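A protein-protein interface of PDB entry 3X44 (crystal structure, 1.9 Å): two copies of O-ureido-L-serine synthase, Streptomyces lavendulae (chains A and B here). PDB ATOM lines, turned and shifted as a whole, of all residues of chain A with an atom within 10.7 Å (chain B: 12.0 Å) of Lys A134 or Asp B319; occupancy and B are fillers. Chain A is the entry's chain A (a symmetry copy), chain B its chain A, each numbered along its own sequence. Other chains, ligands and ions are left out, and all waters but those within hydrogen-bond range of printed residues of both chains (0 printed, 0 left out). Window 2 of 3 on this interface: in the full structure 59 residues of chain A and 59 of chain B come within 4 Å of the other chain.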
ATOM      1  N   THR A  65      22.401 -28.772  19.594  1.00  0.00           N
ATOM      2  CA  THR A  65      21.141 -28.036  19.587  1.00  0.00           C
ATOM      3  C   THR A  65      20.200 -28.500  18.472  1.00  0.00           C
ATOM      4  O   THR A  65      20.599 -28.617  17.316  1.00  0.00           O
ATOM      5  CB  THR A  65      21.394 -26.518  19.424  1.00  0.00           C
ATOM      6  OG1 THR A  65      22.059 -26.011  20.592  1.00  0.00           O
ATOM      7  CG2 THR A  65      20.077 -25.779  19.230  1.00  0.00           C
ATOM      8  N   VAL A  67      16.620 -27.823  16.376  1.00  0.00           N
ATOM      9  CA  VAL A  67      15.669 -26.773  16.029  1.00  0.00           C
ATOM     10  C   VAL A  67      14.575 -27.337  15.136  1.00  0.00           C
ATOM     11  O   VAL A  67      14.846 -28.141  14.239  1.00  0.00           O
ATOM     12  CB  VAL A  67      16.353 -25.588  15.300  1.00  0.00           C
ATOM     13  CG1 VAL A  67      16.824 -26.017  13.915  1.00  0.00           C
ATOM     14  CG2 VAL A  67      15.380 -24.422  15.188  1.00  0.00           C
ATOM     15  N   LEU A 126      11.153 -22.159   6.987  1.00  0.00           N
ATOM     16  CA  LEU A 126      12.188 -21.330   6.404  1.00  0.00           C
ATOM     17  C   LEU A 126      13.009 -20.711   7.520  1.00  0.00           C
ATOM     18  O   LEU A 126      14.235 -20.671   7.447  1.00  0.00           O
ATOM     19  CB  LEU A 126      11.562 -20.249   5.529  1.00  0.00           C
ATOM     20  CG  LEU A 126      11.330 -20.764   4.105  1.00  0.00           C
ATOM     21  CD1 LEU A 126      10.360 -19.860   3.361  1.00  0.00           C
ATOM     22  CD2 LEU A 126      12.671 -20.837   3.377  1.00  0.00           C
ATOM     23  N   ILE A 127      12.333 -20.246   8.565  1.00  0.00           N
ATOM     24  CA  ILE A 127      13.028 -19.640   9.695  1.00  0.00           C
ATOM     25  C   ILE A 127      13.899 -20.696  10.357  1.00  0.00           C
ATOM     26  O   ILE A 127      15.073 -20.463  10.642  1.00  0.00           O
ATOM     27  CB  ILE A 127      12.038 -19.075  10.741  1.00  0.00           C
ATOM     28  CG1 ILE A 127      11.328 -17.848  10.169  1.00  0.00           C
ATOM     29  CG2 ILE A 127      12.781 -18.691  12.017  1.00  0.00           C
ATOM     30  CD1 ILE A 127      10.164 -17.367  11.014  1.00  0.00           C
ATOM     31  N   ALA A 128      13.317 -21.863  10.596  1.00  0.00           N
ATOM     32  CA  ALA A 128      14.042 -22.965  11.211  1.00  0.00           C
ATOM     33  C   ALA A 128      15.282 -23.309  10.377  1.00  0.00           C
ATOM     34  O   ALA A 128      16.369 -23.516  10.916  1.00  0.00           O
ATOM     35  CB  ALA A 128      13.137 -24.175  11.323  1.00  0.00           C
ATOM     36  N   ASP A 129      15.115 -23.358   9.059  1.00  0.00           N
ATOM     37  CA  ASP A 129      16.219 -23.685   8.163  1.00  0.00           C
ATOM     38  C   ASP A 129      17.314 -22.627   8.224  1.00  0.00           C
ATOM     39  O   ASP A 129      18.502 -22.948   8.275  1.00  0.00           O
ATOM     40  CB  ASP A 129      15.706 -23.822   6.721  1.00  0.00           C
ATOM     41  CG  ASP A 129      14.924 -25.112   6.495  1.00  0.00           C
ATOM     42  OD1 ASP A 129      14.180 -25.190   5.497  1.00  0.00           O
ATOM     43  OD2 ASP A 129      15.051 -26.046   7.312  1.00  0.00           O
ATOM     44  N   GLU A 130      16.905 -21.364   8.219  1.00  0.00           N
ATOM     45  CA  GLU A 130      17.843 -20.254   8.275  1.00  0.00           C
ATOM     46  C   GLU A 130      18.656 -20.275   9.567  1.00  0.00           C
ATOM     47  O   GLU A 130      19.864 -20.025   9.551  1.00  0.00           O
ATOM     48  CB  GLU A 130      17.091 -18.925   8.150  1.00  0.00           C
ATOM     49  CG  GLU A 130      16.664 -18.591   6.718  1.00  0.00           C
ATOM     50  CD  GLU A 130      15.823 -17.321   6.618  1.00  0.00           C
ATOM     51  OE1 GLU A 130      15.560 -16.676   7.661  1.00  0.00           O
ATOM     52  OE2 GLU A 130      15.423 -16.968   5.487  1.00  0.00           O
ATOM     53  N   LEU A 131      17.997 -20.575  10.685  1.00  0.00           N
ATOM     54  CA  LEU A 131      18.680 -20.624  11.975  1.00  0.00           C
ATOM     55  C   LEU A 131      19.712 -21.737  12.003  1.00  0.00           C
ATOM     56  O   LEU A 131      20.813 -21.571  12.524  1.00  0.00           O
ATOM     57  CB  LEU A 131      17.682 -20.868  13.106  1.00  0.00           C
ATOM     58  CG  LEU A 131      16.655 -19.771  13.348  1.00  0.00           C
ATOM     59  CD1 LEU A 131      15.600 -20.271  14.325  1.00  0.00           C
ATOM     60  CD2 LEU A 131      17.362 -18.528  13.876  1.00  0.00           C
ATOM     61  N   ALA A 132      19.339 -22.880  11.447  1.00  0.00           N
ATOM     62  CA  ALA A 132      20.231 -24.024  11.417  1.00  0.00           C
ATOM     63  C   ALA A 132      21.492 -23.708  10.626  1.00  0.00           C
ATOM     64  O   ALA A 132      22.600 -23.994  11.073  1.00  0.00           O
ATOM     65  CB  ALA A 132      19.516 -25.226  10.810  1.00  0.00           C
ATOM     66  N   GLU A 133      21.320 -23.108   9.452  1.00  0.00           N
ATOM     67  CA  GLU A 133      22.449 -22.775   8.593  1.00  0.00           C
ATOM     68  C   GLU A 133      23.381 -21.760   9.226  1.00  0.00           C
ATOM     69  O   GLU A 133      24.591 -21.789   9.005  1.00  0.00           O
ATOM     70  CB  GLU A 133      21.951 -22.229   7.260  1.00  0.00           C
ATOM     71  CG  GLU A 133      20.929 -23.103   6.574  1.00  0.00           C
ATOM     72  CD  GLU A 133      20.525 -22.543   5.230  1.00  0.00           C
ATOM     73  OE1 GLU A 133      19.378 -22.793   4.795  1.00  0.00           O
ATOM     74  OE2 GLU A 133      21.360 -21.846   4.612  1.00  0.00           O
ATOM     75  N   LYS A 134      22.809 -20.862  10.013  1.00  0.00           N
ATOM     76  CA  LYS A 134      23.583 -19.826  10.668  1.00  0.00           C
ATOM     77  C   LYS A 134      24.335 -20.328  11.893  1.00  0.00           C
ATOM     78  O   LYS A 134      25.463 -19.903  12.147  1.00  0.00           O
ATOM     79  CB  LYS A 134      22.664 -18.670  11.071  1.00  0.00           C
ATOM     80  CG  LYS A 134      23.392 -17.372  11.376  1.00  0.00           C
ATOM     81  CD  LYS A 134      22.441 -16.319  11.913  1.00  0.00           C
ATOM     82  CE  LYS A 134      23.166 -15.014  12.206  1.00  0.00           C
ATOM     83  NZ  LYS A 134      22.210 -13.926  12.562  1.00  0.00           N
ATOM     84  N   TYR A 135      23.725 -21.242  12.640  1.00  0.00           N
ATOM     85  CA  TYR A 135      24.348 -21.750  13.857  1.00  0.00           C
ATOM     86  C   TYR A 135      24.747 -23.223  13.868  1.00  0.00           C
ATOM     87  O   TYR A 135      25.354 -23.691  14.833  1.00  0.00           O
ATOM     88  CB  TYR A 135      23.438 -21.443  15.043  1.00  0.00           C
ATOM     89  CG  TYR A 135      23.041 -19.985  15.104  1.00  0.00           C
ATOM     90  CD1 TYR A 135      21.796 -19.559  14.638  1.00  0.00           C
ATOM     91  CD2 TYR A 135      23.925 -19.027  15.608  1.00  0.00           C
ATOM     92  CE1 TYR A 135      21.442 -18.210  14.673  1.00  0.00           C
ATOM     93  CE2 TYR A 135      23.575 -17.678  15.645  1.00  0.00           C
ATOM     94  CZ  TYR A 135      22.336 -17.280  15.178  1.00  0.00           C
ATOM     95  OH  TYR A 135      21.994 -15.950  15.223  1.00  0.00           O
ATOM     96  N   GLY A 136      24.407 -23.948  12.807  1.00  0.00           N
ATOM     97  CA  GLY A 136      24.763 -25.356  12.716  1.00  0.00           C
ATOM     98  C   GLY A 136      23.893 -26.333  13.494  1.00  0.00           C
ATOM     99  O   GLY A 136      24.247 -27.504  13.642  1.00  0.00           O
ATOM    100  N   TRP A 137      22.754 -25.860  13.986  1.00  0.00           N
ATOM    101  CA  TRP A 137      21.847 -26.707  14.756  1.00  0.00           C
ATOM    102  C   TRP A 137      21.272 -27.838  13.918  1.00  0.00           C
ATOM    103  O   TRP A 137      21.195 -27.735  12.693  1.00  0.00           O
ATOM    104  CB  TRP A 137      20.708 -25.862  15.315  1.00  0.00           C
ATOM    105  CG  TRP A 137      21.174 -24.717  16.135  1.00  0.00           C
ATOM    106  CD1 TRP A 137      22.385 -24.589  16.762  1.00  0.00           C
ATOM    107  CD2 TRP A 137      20.425 -23.543  16.462  1.00  0.00           C
ATOM    108  NE1 TRP A 137      22.430 -23.406  17.462  1.00  0.00           N
ATOM    109  CE2 TRP A 137      21.241 -22.745  17.296  1.00  0.00           C
ATOM    110  CE3 TRP A 137      19.141 -23.088  16.133  1.00  0.00           C
ATOM    111  CZ2 TRP A 137      20.814 -21.517  17.806  1.00  0.00           C
ATOM    112  CZ3 TRP A 137      18.717 -21.866  16.640  1.00  0.00           C
ATOM    113  CH2 TRP A 137      19.553 -21.094  17.469  1.00  0.00           C
ATOM    114  N   PHE A 138      20.875 -28.920  14.581  1.00  0.00           N
ATOM    115  CA  PHE A 138      20.296 -30.073  13.894  1.00  0.00           C
ATOM    116  C   PHE A 138      18.826 -29.786  13.616  1.00  0.00           C
ATOM    117  O   PHE A 138      18.123 -29.252  14.474  1.00  0.00           O
ATOM    118  CB  PHE A 138      20.434 -31.326  14.768  1.00  0.00           C
ATOM    119  CG  PHE A 138      19.666 -32.517  14.261  1.00  0.00           C
ATOM    120  CD1 PHE A 138      20.142 -33.269  13.188  1.00  0.00           C
ATOM    121  CD2 PHE A 138      18.465 -32.893  14.860  1.00  0.00           C
ATOM    122  CE1 PHE A 138      19.431 -34.376  12.719  1.00  0.00           C
ATOM    123  CE2 PHE A 138      17.751 -33.994  14.400  1.00  0.00           C
ATOM    124  CZ  PHE A 138      18.235 -34.737  13.327  1.00  0.00           C
ATOM    125  N   ARG A 139      18.371 -30.124  12.414  1.00  0.00           N
ATOM    126  CA  ARG A 139      16.980 -29.914  12.033  1.00  0.00           C
ATOM    127  C   ARG A 139      16.242 -31.246  12.097  1.00  0.00           C
ATOM    128  O   ARG A 139      16.659 -32.219  11.474  1.00  0.00           O
ATOM    129  CB  ARG A 139      16.883 -29.361  10.604  1.00  0.00           C
ATOM    130  CG  ARG A 139      17.348 -27.925  10.436  1.00  0.00           C
ATOM    131  CD  ARG A 139      16.212 -26.939  10.667  1.00  0.00           C
ATOM    132  NE  ARG A 139      15.092 -27.159   9.754  1.00  0.00           N
ATOM    133  CZ  ARG A 139      13.909 -27.633  10.128  1.00  0.00           C
ATOM    134  NH1 ARG A 139      13.687 -27.938  11.401  1.00  0.00           N
ATOM    135  NH2 ARG A 139      12.949 -27.803   9.230  1.00  0.00           N
ATOM    136  N   ARG A 141      13.328 -31.743  10.895  1.00  0.00           N
ATOM    137  CA  ARG A 141      12.617 -31.854   9.611  1.00  0.00           C
ATOM    138  C   ARG A 141      11.458 -32.829   9.719  1.00  0.00           C
ATOM    139  O   ARG A 141      11.359 -33.767   8.934  1.00  0.00           O
ATOM    140  CB  ARG A 141      13.565 -32.323   8.500  1.00  0.00           C
ATOM    141  CG  ARG A 141      14.886 -31.601   8.469  1.00  0.00           C
ATOM    142  CD  ARG A 141      15.521 -31.665   7.086  1.00  0.00           C
ATOM    143  NE  ARG A 141      16.565 -30.652   6.946  1.00  0.00           N
ATOM    144  CZ  ARG A 141      16.352 -29.397   6.554  1.00  0.00           C
ATOM    145  NH1 ARG A 141      15.125 -28.988   6.252  1.00  0.00           N
ATOM    146  NH2 ARG A 141      17.365 -28.546   6.472  1.00  0.00           N
ATOM    147  N   ASP B 311      12.587 -15.332  21.769  1.00  0.00           N
ATOM    148  CA  ASP B 311      13.955 -15.194  22.272  1.00  0.00           C
ATOM    149  C   ASP B 311      14.831 -14.336  21.362  1.00  0.00           C
ATOM    150  O   ASP B 311      15.970 -14.698  21.060  1.00  0.00           O
ATOM    151  CB  ASP B 311      14.600 -16.572  22.435  1.00  0.00           C
ATOM    152  CG  ASP B 311      14.133 -17.289  23.684  1.00  0.00           C
ATOM    153  OD1 ASP B 311      13.870 -16.602  24.693  1.00  0.00           O
ATOM    154  OD2 ASP B 311      14.029 -18.537  23.658  1.00  0.00           O
ATOM    155  N   ASP B 312      14.298 -13.198  20.933  1.00  0.00           N
ATOM    156  CA  ASP B 312      15.034 -12.296  20.056  1.00  0.00           C
ATOM    157  C   ASP B 312      16.364 -11.885  20.687  1.00  0.00           C
ATOM    158  O   ASP B 312      17.387 -11.796  20.003  1.00  0.00           O
ATOM    159  CB  ASP B 312      14.191 -11.050  19.761  1.00  0.00           C
ATOM    160  CG  ASP B 312      12.918 -11.374  18.994  1.00  0.00           C
ATOM    161  OD1 ASP B 312      11.942 -10.602  19.109  1.00  0.00           O
ATOM    162  OD2 ASP B 312      12.893 -12.398  18.276  1.00  0.00           O
ATOM    163  N   ALA B 313      16.338 -11.647  21.993  1.00  0.00           N
ATOM    164  CA  ALA B 313      17.530 -11.240  22.728  1.00  0.00           C
ATOM    165  C   ALA B 313      18.578 -12.345  22.733  1.00  0.00           C
ATOM    166  O   ALA B 313      19.758 -12.096  22.480  1.00  0.00           O
ATOM    167  CB  ALA B 313      17.161 -10.862  24.157  1.00  0.00           C
ATOM    168  N   TRP B 314      18.145 -13.565  23.026  1.00  0.00           N
ATOM    169  CA  TRP B 314      19.063 -14.692  23.051  1.00  0.00           C
ATOM    170  C   TRP B 314      19.726 -14.845  21.686  1.00  0.00           C
ATOM    171  O   TRP B 314      20.950 -14.969  21.589  1.00  0.00           O
ATOM    172  CB  TRP B 314      18.321 -15.978  23.413  1.00  0.00           C
ATOM    173  CG  TRP B 314      19.203 -17.187  23.385  1.00  0.00           C
ATOM    174  CD1 TRP B 314      20.260 -17.453  24.211  1.00  0.00           C
ATOM    175  CD2 TRP B 314      19.114 -18.293  22.480  1.00  0.00           C
ATOM    176  NE1 TRP B 314      20.834 -18.656  23.876  1.00  0.00           N
ATOM    177  CE2 TRP B 314      20.151 -19.193  22.816  1.00  0.00           C
ATOM    178  CE3 TRP B 314      18.259 -18.613  21.416  1.00  0.00           C
ATOM    179  CZ2 TRP B 314      20.356 -20.394  22.126  1.00  0.00           C
ATOM    180  CZ3 TRP B 314      18.462 -19.805  20.728  1.00  0.00           C
ATOM    181  CH2 TRP B 314      19.504 -20.681  21.087  1.00  0.00           C
ATOM    182  N   LEU B 315      18.912 -14.829  20.633  1.00  0.00           N
ATOM    183  CA  LEU B 315      19.414 -14.965  19.271  1.00  0.00           C
ATOM    184  C   LEU B 315      20.492 -13.927  18.975  1.00  0.00           C
ATOM    185  O   LEU B 315      21.506 -14.230  18.344  1.00  0.00           O
ATOM    186  CB  LEU B 315      18.269 -14.816  18.269  1.00  0.00           C
ATOM    187  CG  LEU B 315      17.375 -16.043  18.103  1.00  0.00           C
ATOM    188  CD1 LEU B 315      16.169 -15.682  17.256  1.00  0.00           C
ATOM    189  CD2 LEU B 315      18.170 -17.168  17.464  1.00  0.00           C
ATOM    190  N   ALA B 316      20.266 -12.700  19.429  1.00  0.00           N
ATOM    191  CA  ALA B 316      21.229 -11.631  19.218  1.00  0.00           C
ATOM    192  C   ALA B 316      22.484 -11.915  20.044  1.00  0.00           C
ATOM    193  O   ALA B 316      23.606 -11.723  19.575  1.00  0.00           O
ATOM    194  CB  ALA B 316      20.620 -10.291  19.621  1.00  0.00           C
ATOM    195  N   SER B 317      22.282 -12.384  21.271  1.00  0.00           N
ATOM    196  CA  SER B 317      23.388 -12.699  22.166  1.00  0.00           C
ATOM    197  C   SER B 317      24.363 -13.688  21.532  1.00  0.00           C
ATOM    198  O   SER B 317      25.518 -13.786  21.946  1.00  0.00           O
ATOM    199  CB  SER B 317      22.848 -13.282  23.472  1.00  0.00           C
ATOM    200  OG  SER B 317      23.113 -12.417  24.562  1.00  0.00           O
ATOM    201  N   LEU B 318      23.890 -14.417  20.526  1.00  0.00           N
ATOM    202  CA  LEU B 318      24.712 -15.408  19.839  1.00  0.00           C
ATOM    203  C   LEU B 318      25.689 -14.776  18.852  1.00  0.00           C
ATOM    204  O   LEU B 318      26.892 -15.035  18.906  1.00  0.00           O
ATOM    205  CB  LEU B 318      23.821 -16.410  19.100  1.00  0.00           C
ATOM    206  CG  LEU B 318      22.811 -17.190  19.945  1.00  0.00           C
ATOM    207  CD1 LEU B 318      21.869 -17.958  19.034  1.00  0.00           C
ATOM    208  CD2 LEU B 318      23.541 -18.137  20.883  1.00  0.00           C
ATOM    209  N   ASP B 319      25.167 -13.950  17.949  1.00  0.00           N
ATOM    210  CA  ASP B 319      25.994 -13.290  16.943  1.00  0.00           C
ATOM    211  C   ASP B 319      27.217 -12.597  17.541  1.00  0.00           C
ATOM    212  O   ASP B 319      28.326 -12.707  17.014  1.00  0.00           O
ATOM    213  CB  ASP B 319      25.157 -12.267  16.174  1.00  0.00           C
ATOM    214  CG  ASP B 319      24.130 -12.917  15.273  1.00  0.00           C
ATOM    215  OD1 ASP B 319      23.211 -13.576  15.801  1.00  0.00           O
ATOM    216  OD2 ASP B 319      24.244 -12.769  14.037  1.00  0.00           O
ATOM    217  N   THR B 320      27.005 -11.889  18.645  1.00  0.00           N
ATOM    218  CA  THR B 320      28.077 -11.165  19.317  1.00  0.00           C
ATOM    219  C   THR B 320      29.072 -12.087  20.019  1.00  0.00           C
ATOM    220  O   THR B 320      29.227 -13.252  19.655  1.00  0.00           O
ATOM    221  CB  THR B 320      27.504 -10.187  20.362  1.00  0.00           C
ATOM    222  OG1 THR B 320      26.664 -10.902  21.278  1.00  0.00           O
ATOM    223  CG2 THR B 320      26.692  -9.096  19.680  1.00  0.00           C
ATOM    224  N   GLY B 321      29.748 -11.541  21.025  1.00  0.00           N
ATOM    225  CA  GLY B 321      30.720 -12.301  21.785  1.00  0.00           C
ATOM    226  C   GLY B 321      30.643 -11.913  23.249  1.00  0.00           C
ATOM    227  O   GLY B 321      31.664 -11.741  23.917  1.00  0.00           O
ATOM    228  N   SER B 322      29.416 -11.773  23.741  1.00  0.00           N
ATOM    229  CA  SER B 322      29.153 -11.398  25.127  1.00  0.00           C
ATOM    230  C   SER B 322      29.972 -12.201  26.135  1.00  0.00           C
ATOM    231  O   SER B 322      30.025 -11.784  27.313  1.00  0.00           O
ATOM    232  CB  SER B 322      27.664 -11.568  25.426  1.00  0.00           C
ATOM    233  OG  SER B 322      26.969 -12.016  24.275  1.00  0.00           O
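The side-chain carboxylate (OD2) of Asp B319 lies within salt-bridge range of the side-chain amino group (NZ) of Lys A134 (2.8 Å). OH of Tyr A135 sits at hydrogen-bond distance from OD1 of Asp B319.
The side-chain amino group (NZ) of Lys A134 lies within hydrogen-bond range of the side-chain hydroxyl (OH) of Tyr A135 (3.4 Å). O of Ala A132 is in hydrogen-bond range of N of Trp A137 (3.5 Å).
Leu A131 touches Leu B315 (CD2 to CD2, 3.9 Å). Tyr A135 touches Leu B315 (OH to O, 3.6 Å). CB of Leu B318 touches CE2 of Tyr A135, 3.7 Å away. Trp A137 touches Trp B314 (CZ2 to CH2, 3.6 Å). Leu B318 touches Trp A137 (CD1 to CZ2, 3.9 Å).
No residue of chain B comes within 4 Å of Glu A133. Of chain B, only Asp B319 (2.8 Å) comes within 4 Å of Lys A134. Tyr A135 touches three residues of chain B. Of the printed residues of chain B, Trp A137 touches Trp B314 (3.6 Å) and Leu B318 (3.9 Å). Arg A139 touches none of the printed residues of chain B. Of the printed residues of chain A, Trp B314 touches Trp A137. No residue of chain A comes within 4 Å of Ala B316. Leu B318 touches just these residues of chain A: Tyr A135 (3.7 Å) and Trp A137 (3.9 Å). Asp B319 touches two residues of chain A. No residue of chain A comes within 4 Å of Thr B320.
Hydrophobic or aromatic side chains of chain A that line the printed part of chain B: Leu A131, Tyr A135 and Trp A137. Of the 12 printed residues of chain B, 4 touch a printed residue of chain A. Printed residues of chain B that touch a printed residue of chain A: Trp B314, Leu B315, Leu B318 and Asp B319. Hydrophobic or aromatic side chains of chain B that line the printed part of chain A: Trp B314, Leu B315 and Leu B318. Among the printed residues, Asp or Glu carboxylates within 4 Å of a Lys or Arg side-chain nitrogen of the other chain: Lys A134 with Asp B319 (2.8 Å).
No position is printed for both chains. Of the 7 pairs that touch across the chains among the printed residues, none has its exchanged pair printed and touching as well.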
